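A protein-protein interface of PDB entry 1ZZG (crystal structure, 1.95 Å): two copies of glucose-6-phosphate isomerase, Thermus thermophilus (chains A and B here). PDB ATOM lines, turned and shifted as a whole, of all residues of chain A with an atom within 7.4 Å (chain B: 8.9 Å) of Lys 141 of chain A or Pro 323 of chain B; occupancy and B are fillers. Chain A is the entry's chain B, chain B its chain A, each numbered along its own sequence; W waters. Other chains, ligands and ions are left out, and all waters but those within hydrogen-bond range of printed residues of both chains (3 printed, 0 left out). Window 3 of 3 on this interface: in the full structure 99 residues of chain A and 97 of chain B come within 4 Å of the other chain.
O of Lys 337 of chain B is in hydrogen-bond range of N of Ile 322 of chain B (2.8 Å). The backbone carbonyl oxygen of Ile 322 of chain B is in hydrogen-bond range of the backbone NH of Gly 336 of chain B (3.0 Å).
No position is printed for both chains.
Lys 141 of chain A touches just one residue of chain B: Pro 323 (3.7 Å). Printed residues of chain A within 4 Å of Pro 323 of chain B: Ala 137, Val 138 and Lys 141. Of the printed residues of chain A, Val 325 of chain B touches Ala 137 (3.6 Å) and Leu 140 (3.5 Å). Printed residues of chain A within 4 Å of Glu 326 of chain B: Lys 144. The nearest residue of chain B that does not touch Lys 141 of chain A is Glu 321 of chain B (5.9 Å).
CB of Ala 331 of chain B touches CD1 of Leu 133 of chain A, at 3.9 Å. CB of Ala 134 of chain A touches CD1 of Ile 322 of chain B (3.9 Å). CD1 of Leu 334 of chain B touches N of Ala 134 of chain A (3.95 Å). CG2 of Ile 322 of chain B touches CB of Ala 137 of chain A (3.8 Å). Ala 137 of chain A touches Pro 323 of chain B (O to CG, 3.2 Å). Ala 137 of chain A touches Val 325 of chain B (CB to CG2, 3.6 Å). Val 138 of chain A touches Pro 323 of chain B. Val 325 of chain B touches Leu 140 of chain A. CD of Lys 141 of chain A touches CB of Pro 323 of chain B, 3.7 Å away. Glu 326 of chain B touches Lys 144 of chain A (CG to NZ, 3.5 Å).
Of the 16 printed residues of chain A, 7 touch a printed residue of chain B. Printed residues of chain A that touch a printed residue of chain B: Leu 133, Ala 134, Ala 137, Val 138, Leu 140, Lys 141 and Lys 144. Among the printed residues, 10 pairs touch across the chains.
Water W2 bridges O of Glu 326 of chain B (2.5 Å) and NZ of Lys 144 of chain A (3.0 Å). Water W3 lies within hydrogen-bond range of NZ of Lys 144 of chain A (2.9 Å) and N of Glu 326 of chain B (3.0 Å). Water W1 lies within hydrogen-bond range of O of Ala 137 of chain A (2.9 Å), O of Glu 324 of chain B (3.2 Å) and N of Lys 141 of chain A (3.5 Å).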
ATOM      1  N   LEU A 110      10.755   5.877  34.050  1.00  0.00           N
ATOM      2  CA  LEU A 110       9.680   5.300  33.252  1.00  0.00           C
ATOM      3  C   LEU A 110       9.590   3.788  33.440  1.00  0.00           C
ATOM      4  O   LEU A 110       8.514   3.202  33.313  1.00  0.00           O
ATOM      5  CB  LEU A 110       9.893   5.620  31.768  1.00  0.00           C
ATOM      6  CG  LEU A 110       9.988   7.098  31.375  1.00  0.00           C
ATOM      7  CD1 LEU A 110      10.157   7.226  29.860  1.00  0.00           C
ATOM      8  CD2 LEU A 110       8.734   7.826  31.834  1.00  0.00           C
ATOM      9  N   LEU A 133       9.435  21.330  28.725  1.00  0.00           N
ATOM     10  CA  LEU A 133       8.544  20.896  27.659  1.00  0.00           C
ATOM     11  C   LEU A 133       8.997  19.525  27.163  1.00  0.00           C
ATOM     12  O   LEU A 133       8.174  18.647  26.926  1.00  0.00           O
ATOM     13  CB  LEU A 133       8.540  21.897  26.497  1.00  0.00           C
ATOM     14  CG  LEU A 133       7.809  23.222  26.745  1.00  0.00           C
ATOM     15  CD1 LEU A 133       7.901  24.113  25.512  1.00  0.00           C
ATOM     16  CD2 LEU A 133       6.352  22.940  27.091  1.00  0.00           C
ATOM     17  N   ALA A 134      10.309  19.345  27.027  1.00  0.00           N
ATOM     18  CA  ALA A 134      10.864  18.076  26.555  1.00  0.00           C
ATOM     19  C   ALA A 134      10.517  16.944  27.511  1.00  0.00           C
ATOM     20  O   ALA A 134      10.063  15.872  27.095  1.00  0.00           O
ATOM     21  CB  ALA A 134      12.384  18.188  26.407  1.00  0.00           C
ATOM     22  N   GLY A 135      10.733  17.187  28.797  1.00  0.00           N
ATOM     23  CA  GLY A 135      10.439  16.175  29.792  1.00  0.00           C
ATOM     24  C   GLY A 135       8.958  15.868  29.854  1.00  0.00           C
ATOM     25  O   GLY A 135       8.563  14.713  30.025  1.00  0.00           O
ATOM     26  N   LEU A 136       8.133  16.899  29.717  1.00  0.00           N
ATOM     27  CA  LEU A 136       6.688  16.706  29.766  1.00  0.00           C
ATOM     28  C   LEU A 136       6.235  15.812  28.615  1.00  0.00           C
ATOM     29  O   LEU A 136       5.483  14.859  28.825  1.00  0.00           O
ATOM     30  CB  LEU A 136       5.961  18.058  29.706  1.00  0.00           C
ATOM     31  CG  LEU A 136       4.425  18.017  29.663  1.00  0.00           C
ATOM     32  CD1 LEU A 136       3.881  17.239  30.857  1.00  0.00           C
ATOM     33  CD2 LEU A 136       3.885  19.440  29.665  1.00  0.00           C
ATOM     34  N   ALA A 137       6.707  16.114  27.407  1.00  0.00           N
ATOM     35  CA  ALA A 137       6.346  15.341  26.219  1.00  0.00           C
ATOM     36  C   ALA A 137       6.631  13.861  26.438  1.00  0.00           C
ATOM     37  O   ALA A 137       5.826  13.004  26.080  1.00  0.00           O
ATOM     38  CB  ALA A 137       7.122  15.848  24.997  1.00  0.00           C
ATOM     39  N   VAL A 138       7.785  13.566  27.024  1.00  0.00           N
ATOM     40  CA  VAL A 138       8.164  12.187  27.287  1.00  0.00           C
ATOM     41  C   VAL A 138       7.227  11.535  28.292  1.00  0.00           C
ATOM     42  O   VAL A 138       6.775  10.407  28.087  1.00  0.00           O
ATOM     43  CB  VAL A 138       9.615  12.100  27.818  1.00  0.00           C
ATOM     44  CG1 VAL A 138       9.926  10.683  28.272  1.00  0.00           C
ATOM     45  CG2 VAL A 138      10.584  12.527  26.730  1.00  0.00           C
ATOM     46  N   PHE A 139       6.927  12.236  29.382  1.00  0.00           N
ATOM     47  CA  PHE A 139       6.048  11.666  30.393  1.00  0.00           C
ATOM     48  C   PHE A 139       4.592  11.568  29.949  1.00  0.00           C
ATOM     49  O   PHE A 139       3.850  10.715  30.439  1.00  0.00           O
ATOM     50  CB  PHE A 139       6.154  12.439  31.713  1.00  0.00           C
ATOM     51  CG  PHE A 139       7.077  11.792  32.704  1.00  0.00           C
ATOM     52  CD1 PHE A 139       8.447  12.048  32.680  1.00  0.00           C
ATOM     53  CD2 PHE A 139       6.588  10.862  33.613  1.00  0.00           C
ATOM     54  CE1 PHE A 139       9.312  11.380  33.547  1.00  0.00           C
ATOM     55  CE2 PHE A 139       7.445  10.188  34.484  1.00  0.00           C
ATOM     56  CZ  PHE A 139       8.809  10.447  34.449  1.00  0.00           C
ATOM     57  N   LEU A 140       4.192  12.439  29.024  1.00  0.00           N
ATOM     58  CA  LEU A 140       2.827  12.417  28.499  1.00  0.00           C
ATOM     59  C   LEU A 140       2.606  11.129  27.713  1.00  0.00           C
ATOM     60  O   LEU A 140       1.623  10.424  27.934  1.00  0.00           O
ATOM     61  CB  LEU A 140       2.571  13.627  27.591  1.00  0.00           C
ATOM     62  CG  LEU A 140       2.061  14.888  28.295  1.00  0.00           C
ATOM     63  CD1 LEU A 140       1.993  16.048  27.312  1.00  0.00           C
ATOM     64  CD2 LEU A 140       0.683  14.606  28.895  1.00  0.00           C
ATOM     65  N   LYS A 141       3.524  10.825  26.797  1.00  0.00           N
ATOM     66  CA  LYS A 141       3.427   9.609  25.997  1.00  0.00           C
ATOM     67  C   LYS A 141       3.315   8.407  26.932  1.00  0.00           C
ATOM     68  O   LYS A 141       2.490   7.523  26.728  1.00  0.00           O
ATOM     69  CB  LYS A 141       4.666   9.456  25.108  1.00  0.00           C
ATOM     70  CG  LYS A 141       4.654   8.220  24.203  1.00  0.00           C
ATOM     71  CD  LYS A 141       5.975   8.084  23.453  1.00  0.00           C
ATOM     72  CE  LYS A 141       5.963   6.935  22.445  1.00  0.00           C
ATOM     73  NZ  LYS A 141       5.126   7.222  21.242  1.00  0.00           N
ATOM     74  N   TRP A 142       4.155   8.398  27.961  1.00  0.00           N
ATOM     75  CA  TRP A 142       4.192   7.332  28.956  1.00  0.00           C
ATOM     76  C   TRP A 142       2.833   7.194  29.634  1.00  0.00           C
ATOM     77  O   TRP A 142       2.270   6.102  29.699  1.00  0.00           O
ATOM     78  CB  TRP A 142       5.269   7.657  29.998  1.00  0.00           C
ATOM     79  CG  TRP A 142       5.465   6.624  31.068  1.00  0.00           C
ATOM     80  CD1 TRP A 142       5.961   5.362  30.913  1.00  0.00           C
ATOM     81  CD2 TRP A 142       5.219   6.788  32.471  1.00  0.00           C
ATOM     82  NE1 TRP A 142       6.049   4.730  32.134  1.00  0.00           N
ATOM     83  CE2 TRP A 142       5.603   5.584  33.108  1.00  0.00           C
ATOM     84  CE3 TRP A 142       4.723   7.840  33.255  1.00  0.00           C
ATOM     85  CZ2 TRP A 142       5.495   5.399  34.492  1.00  0.00           C
ATOM     86  CZ3 TRP A 142       4.617   7.659  34.634  1.00  0.00           C
ATOM     87  CH2 TRP A 142       5.006   6.447  35.237  1.00  0.00           C
ATOM     88  N   LEU A 143       2.309   8.310  30.132  1.00  0.00           N
ATOM     89  CA  LEU A 143       1.015   8.318  30.804  1.00  0.00           C
ATOM     90  C   LEU A 143      -0.104   7.798  29.905  1.00  0.00           C
ATOM     91  O   LEU A 143      -0.857   6.911  30.293  1.00  0.00           O
ATOM     92  CB  LEU A 143       0.668   9.734  31.274  1.00  0.00           C
ATOM     93  CG  LEU A 143       1.452  10.298  32.463  1.00  0.00           C
ATOM     94  CD1 LEU A 143       1.052  11.751  32.683  1.00  0.00           C
ATOM     95  CD2 LEU A 143       1.173   9.466  33.708  1.00  0.00           C
ATOM     96  N   LYS A 144      -0.216   8.353  28.706  1.00  0.00           N
ATOM     97  CA  LYS A 144      -1.264   7.923  27.791  1.00  0.00           C
ATOM     98  C   LYS A 144      -1.119   6.452  27.425  1.00  0.00           C
ATOM     99  O   LYS A 144      -2.110   5.734  27.310  1.00  0.00           O
ATOM    100  CB  LYS A 144      -1.249   8.782  26.524  1.00  0.00           C
ATOM    101  CG  LYS A 144      -1.555  10.252  26.780  1.00  0.00           C
ATOM    102  CD  LYS A 144      -1.565  11.066  25.492  1.00  0.00           C
ATOM    103  CE  LYS A 144      -1.865  12.529  25.773  1.00  0.00           C
ATOM    104  NZ  LYS A 144      -1.924  13.335  24.523  1.00  0.00           N
ATOM    105  N   ALA A 145       0.119   6.001  27.259  1.00  0.00           N
ATOM    106  CA  ALA A 145       0.381   4.611  26.897  1.00  0.00           C
ATOM    107  C   ALA A 145      -0.078   3.617  27.966  1.00  0.00           C
ATOM    108  O   ALA A 145      -0.574   2.534  27.647  1.00  0.00           O
ATOM    109  CB  ALA A 145       1.872   4.425  26.619  1.00  0.00           C
ATOM    110  N   HIS A 146       0.074   3.991  29.232  1.00  0.00           N
ATOM    111  CA  HIS A 146      -0.289   3.116  30.341  1.00  0.00           C
ATOM    112  C   HIS A 146      -1.670   3.345  30.952  1.00  0.00           C
ATOM    113  O   HIS A 146      -2.287   2.407  31.456  1.00  0.00           O
ATOM    114  CB  HIS A 146       0.759   3.232  31.456  1.00  0.00           C
ATOM    115  CG  HIS A 146       2.110   2.702  31.083  1.00  0.00           C
ATOM    116  ND1 HIS A 146       2.398   1.355  31.054  1.00  0.00           N
ATOM    117  CD2 HIS A 146       3.249   3.337  30.716  1.00  0.00           C
ATOM    118  CE1 HIS A 146       3.655   1.183  30.687  1.00  0.00           C
ATOM    119  NE2 HIS A 146       4.194   2.370  30.475  1.00  0.00           N
ATOM    120  N   LEU A 147      -2.156   4.582  30.911  1.00  0.00           N
ATOM    121  CA  LEU A 147      -3.443   4.904  31.517  1.00  0.00           C
ATOM    122  C   LEU A 147      -4.570   5.213  30.536  1.00  0.00           C
ATOM    123  O   LEU A 147      -5.711   5.434  30.950  1.00  0.00           O
ATOM    124  CB  LEU A 147      -3.270   6.092  32.465  1.00  0.00           C
ATOM    125  CG  LEU A 147      -2.078   6.025  33.424  1.00  0.00           C
ATOM    126  CD1 LEU A 147      -1.965   7.339  34.180  1.00  0.00           C
ATOM    127  CD2 LEU A 147      -2.246   4.863  34.384  1.00  0.00           C
ATOM    128  N   VAL B 320      16.564   8.885  24.186  1.00  0.00           N
ATOM    129  CA  VAL B 320      15.108   8.945  24.204  1.00  0.00           C
ATOM    130  C   VAL B 320      14.607   9.972  23.205  1.00  0.00           C
ATOM    131  O   VAL B 320      14.996  11.143  23.256  1.00  0.00           O
ATOM    132  CB  VAL B 320      14.576   9.351  25.589  1.00  0.00           C
ATOM    133  CG1 VAL B 320      13.074   9.600  25.515  1.00  0.00           C
ATOM    134  CG2 VAL B 320      14.891   8.276  26.599  1.00  0.00           C
ATOM    135  N   GLU B 321      13.744   9.541  22.295  1.00  0.00           N
ATOM    136  CA  GLU B 321      13.201  10.463  21.313  1.00  0.00           C
ATOM    137  C   GLU B 321      12.070  11.242  21.970  1.00  0.00           C
ATOM    138  O   GLU B 321      11.246  10.670  22.682  1.00  0.00           O
ATOM    139  CB  GLU B 321      12.665   9.711  20.089  1.00  0.00           C
ATOM    140  CG  GLU B 321      12.269  10.637  18.945  1.00  0.00           C
ATOM    141  CD  GLU B 321      11.847   9.891  17.696  1.00  0.00           C
ATOM    142  OE1 GLU B 321      12.590   8.984  17.257  1.00  0.00           O
ATOM    143  OE2 GLU B 321      10.777  10.222  17.147  1.00  0.00           O
ATOM    144  N   ILE B 322      12.054  12.553  21.746  1.00  0.00           N
ATOM    145  CA  ILE B 322      11.012  13.408  22.300  1.00  0.00           C
ATOM    146  C   ILE B 322       9.785  13.248  21.400  1.00  0.00           C
ATOM    147  O   ILE B 322       9.792  13.670  20.241  1.00  0.00           O
ATOM    148  CB  ILE B 322      11.453  14.890  22.316  1.00  0.00           C
ATOM    149  CG1 ILE B 322      12.732  15.047  23.153  1.00  0.00           C
ATOM    150  CG2 ILE B 322      10.338  15.761  22.891  1.00  0.00           C
ATOM    151  CD1 ILE B 322      13.374  16.410  23.044  1.00  0.00           C
ATOM    152  N   PRO B 323       8.719  12.623  21.921  1.00  0.00           N
ATOM    153  CA  PRO B 323       7.477  12.394  21.172  1.00  0.00           C
ATOM    154  C   PRO B 323       6.639  13.651  20.957  1.00  0.00           C
ATOM    155  O   PRO B 323       6.663  14.573  21.773  1.00  0.00           O
ATOM    156  CB  PRO B 323       6.759  11.358  22.024  1.00  0.00           C
ATOM    157  CG  PRO B 323       7.127  11.779  23.401  1.00  0.00           C
ATOM    158  CD  PRO B 323       8.610  12.080  23.287  1.00  0.00           C
ATOM    159  N   GLU B 324       5.907  13.697  19.849  1.00  0.00           N
ATOM    160  CA  GLU B 324       5.075  14.858  19.573  1.00  0.00           C
ATOM    161  C   GLU B 324       3.880  14.811  20.515  1.00  0.00           C
ATOM    162  O   GLU B 324       3.433  13.734  20.909  1.00  0.00           O
ATOM    163  CB  GLU B 324       4.620  14.863  18.108  1.00  0.00           C
ATOM    164  CG  GLU B 324       3.612  13.795  17.741  1.00  0.00           C
ATOM    165  CD  GLU B 324       3.329  13.754  16.245  1.00  0.00           C
ATOM    166  OE1 GLU B 324       3.205  14.838  15.630  1.00  0.00           O
ATOM    167  OE2 GLU B 324       3.221  12.637  15.688  1.00  0.00           O
ATOM    168  N   VAL B 325       3.390  15.985  20.900  1.00  0.00           N
ATOM    169  CA  VAL B 325       2.251  16.077  21.804  1.00  0.00           C
ATOM    170  C   VAL B 325       1.106  16.817  21.126  1.00  0.00           C
ATOM    171  O   VAL B 325       1.270  17.949  20.667  1.00  0.00           O
ATOM    172  CB  VAL B 325       2.617  16.834  23.106  1.00  0.00           C
ATOM    173  CG1 VAL B 325       1.401  16.927  24.020  1.00  0.00           C
ATOM    174  CG2 VAL B 325       3.752  16.126  23.817  1.00  0.00           C
ATOM    175  N   GLU B 326      -0.051  16.169  21.058  1.00  0.00           N
ATOM    176  CA  GLU B 326      -1.220  16.788  20.453  1.00  0.00           C
ATOM    177  C   GLU B 326      -1.681  17.920  21.367  1.00  0.00           C
ATOM    178  O   GLU B 326      -1.942  17.701  22.551  1.00  0.00           O
ATOM    179  CB  GLU B 326      -2.343  15.760  20.291  1.00  0.00           C
ATOM    180  CG  GLU B 326      -2.754  15.088  21.591  1.00  0.00           C
ATOM    181  CD  GLU B 326      -3.978  14.205  21.436  1.00  0.00           C
ATOM    182  OE1 GLU B 326      -3.928  13.253  20.625  1.00  0.00           O
ATOM    183  OE2 GLU B 326      -4.990  14.464  22.128  1.00  0.00           O
ATOM    184  N   LEU B 328       0.171  20.714  21.942  1.00  0.00           N
ATOM    185  CA  LEU B 328       1.320  21.436  22.484  1.00  0.00           C
ATOM    186  C   LEU B 328       2.267  21.790  21.340  1.00  0.00           C
ATOM    187  O   LEU B 328       3.448  21.434  21.354  1.00  0.00           O
ATOM    188  CB  LEU B 328       2.047  20.575  23.521  1.00  0.00           C
ATOM    189  CG  LEU B 328       3.093  21.291  24.376  1.00  0.00           C
ATOM    190  CD1 LEU B 328       2.411  22.344  25.234  1.00  0.00           C
ATOM    191  CD2 LEU B 328       3.819  20.281  25.251  1.00  0.00           C
ATOM    192  N   ALA B 331       5.922  23.310  21.307  1.00  0.00           N
ATOM    193  CA  ALA B 331       7.059  22.433  21.574  1.00  0.00           C
ATOM    194  C   ALA B 331       7.398  21.561  20.362  1.00  0.00           C
ATOM    195  O   ALA B 331       8.130  20.575  20.478  1.00  0.00           O
ATOM    196  CB  ALA B 331       6.747  21.546  22.776  1.00  0.00           C
ATOM    197  N   SER B 332       6.874  21.930  19.198  1.00  0.00           N
ATOM    198  CA  SER B 332       7.112  21.157  17.988  1.00  0.00           C
ATOM    199  C   SER B 332       8.565  21.167  17.515  1.00  0.00           C
ATOM    200  O   SER B 332       8.993  20.243  16.822  1.00  0.00           O
ATOM    201  CB  SER B 332       6.197  21.651  16.863  1.00  0.00           C
ATOM    202  OG  SER B 332       6.474  23.003  16.545  1.00  0.00           O
ATOM    203  N   LEU B 334      10.957  20.603  19.213  1.00  0.00           N
ATOM    204  CA  LEU B 334      11.611  19.542  19.969  1.00  0.00           C
ATOM    205  C   LEU B 334      11.176  18.154  19.496  1.00  0.00           C
ATOM    206  O   LEU B 334      11.924  17.186  19.648  1.00  0.00           O
ATOM    207  CB  LEU B 334      11.303  19.684  21.463  1.00  0.00           C
ATOM    208  CG  LEU B 334      11.879  20.902  22.187  1.00  0.00           C
ATOM    209  CD1 LEU B 334      11.259  21.017  23.572  1.00  0.00           C
ATOM    210  CD2 LEU B 334      13.393  20.776  22.277  1.00  0.00           C
ATOM    211  N   PHE B 335       9.973  18.057  18.929  1.00  0.00           N
ATOM    212  CA  PHE B 335       9.464  16.768  18.459  1.00  0.00           C
ATOM    213  C   PHE B 335      10.426  16.157  17.446  1.00  0.00           C
ATOM    214  O   PHE B 335      10.919  16.847  16.552  1.00  0.00           O
ATOM    215  CB  PHE B 335       8.076  16.920  17.809  1.00  0.00           C
ATOM    216  CG  PHE B 335       7.024  17.519  18.714  1.00  0.00           C
ATOM    217  CD1 PHE B 335       7.188  17.545  20.097  1.00  0.00           C
ATOM    218  CD2 PHE B 335       5.852  18.043  18.174  1.00  0.00           C
ATOM    219  CE1 PHE B 335       6.200  18.085  20.929  1.00  0.00           C
ATOM    220  CE2 PHE B 335       4.854  18.586  18.996  1.00  0.00           C
ATOM    221  CZ  PHE B 335       5.030  18.607  20.374  1.00  0.00           C
ATOM    222  N   GLY B 336      10.697  14.863  17.587  1.00  0.00           N
ATOM    223  CA  GLY B 336      11.601  14.203  16.661  1.00  0.00           C
ATOM    224  C   GLY B 336      13.041  14.198  17.135  1.00  0.00           C
ATOM    225  O   GLY B 336      13.796  13.284  16.808  1.00  0.00           O
ATOM    226  N   LYS B 337      13.430  15.219  17.892  1.00  0.00           N
ATOM    227  CA  LYS B 337      14.789  15.303  18.426  1.00  0.00           C
ATOM    228  C   LYS B 337      14.862  14.362  19.622  1.00  0.00           C
ATOM    229  O   LYS B 337      13.828  13.903  20.106  1.00  0.00           O
ATOM    230  CB  LYS B 337      15.098  16.726  18.902  1.00  0.00           C
ATOM    231  CG  LYS B 337      14.697  17.825  17.929  1.00  0.00           C
ATOM    232  CD  LYS B 337      15.394  17.682  16.588  1.00  0.00           C
ATOM    233  CE  LYS B 337      14.964  18.790  15.637  1.00  0.00           C
ATOM    234  NZ  LYS B 337      15.485  18.574  14.261  1.00  0.00           N
ATOM    235  N   THR B 338      16.073  14.080  20.101  1.00  0.00           N
ATOM    236  CA  THR B 338      16.249  13.202  21.260  1.00  0.00           C
ATOM    237  C   THR B 338      16.628  14.023  22.499  1.00  0.00           C
ATOM    238  O   THR B 338      17.039  15.180  22.391  1.00  0.00           O
ATOM    239  CB  THR B 338      17.366  12.154  21.030  1.00  0.00           C
ATOM    240  OG1 THR B 338      18.642  12.807  21.001  1.00  0.00           O
ATOM    241  CG2 THR B 338      17.146  11.414  19.714  1.00  0.00           C
ATOM    242  N   LEU B 339      16.480  13.421  23.674  1.00  0.00           N
ATOM    243  CA  LEU B 339      16.823  14.105  24.914  1.00  0.00           C
ATOM    244  C   LEU B 339      18.318  14.410  24.948  1.00  0.00           C
ATOM    245  O   LEU B 339      18.724  15.508  25.333  1.00  0.00           O
ATOM    246  CB  LEU B 339      16.432  13.254  26.131  1.00  0.00           C
ATOM    247  CG  LEU B 339      14.926  13.168  26.418  1.00  0.00           C
ATOM    248  CD1 LEU B 339      14.677  12.380  27.694  1.00  0.00           C
ATOM    249  CD2 LEU B 339      14.359  14.571  26.552  1.00  0.00           C
HETATM  250  O   HOH W   1       3.829  12.876  24.012  1.00  0.00           O
HETATM  251  O   HOH W   2      -2.632  16.253  24.422  1.00  0.00           O
HETATM  252  O   HOH W   3      -0.198  13.389  22.223  1.00  0.00           O
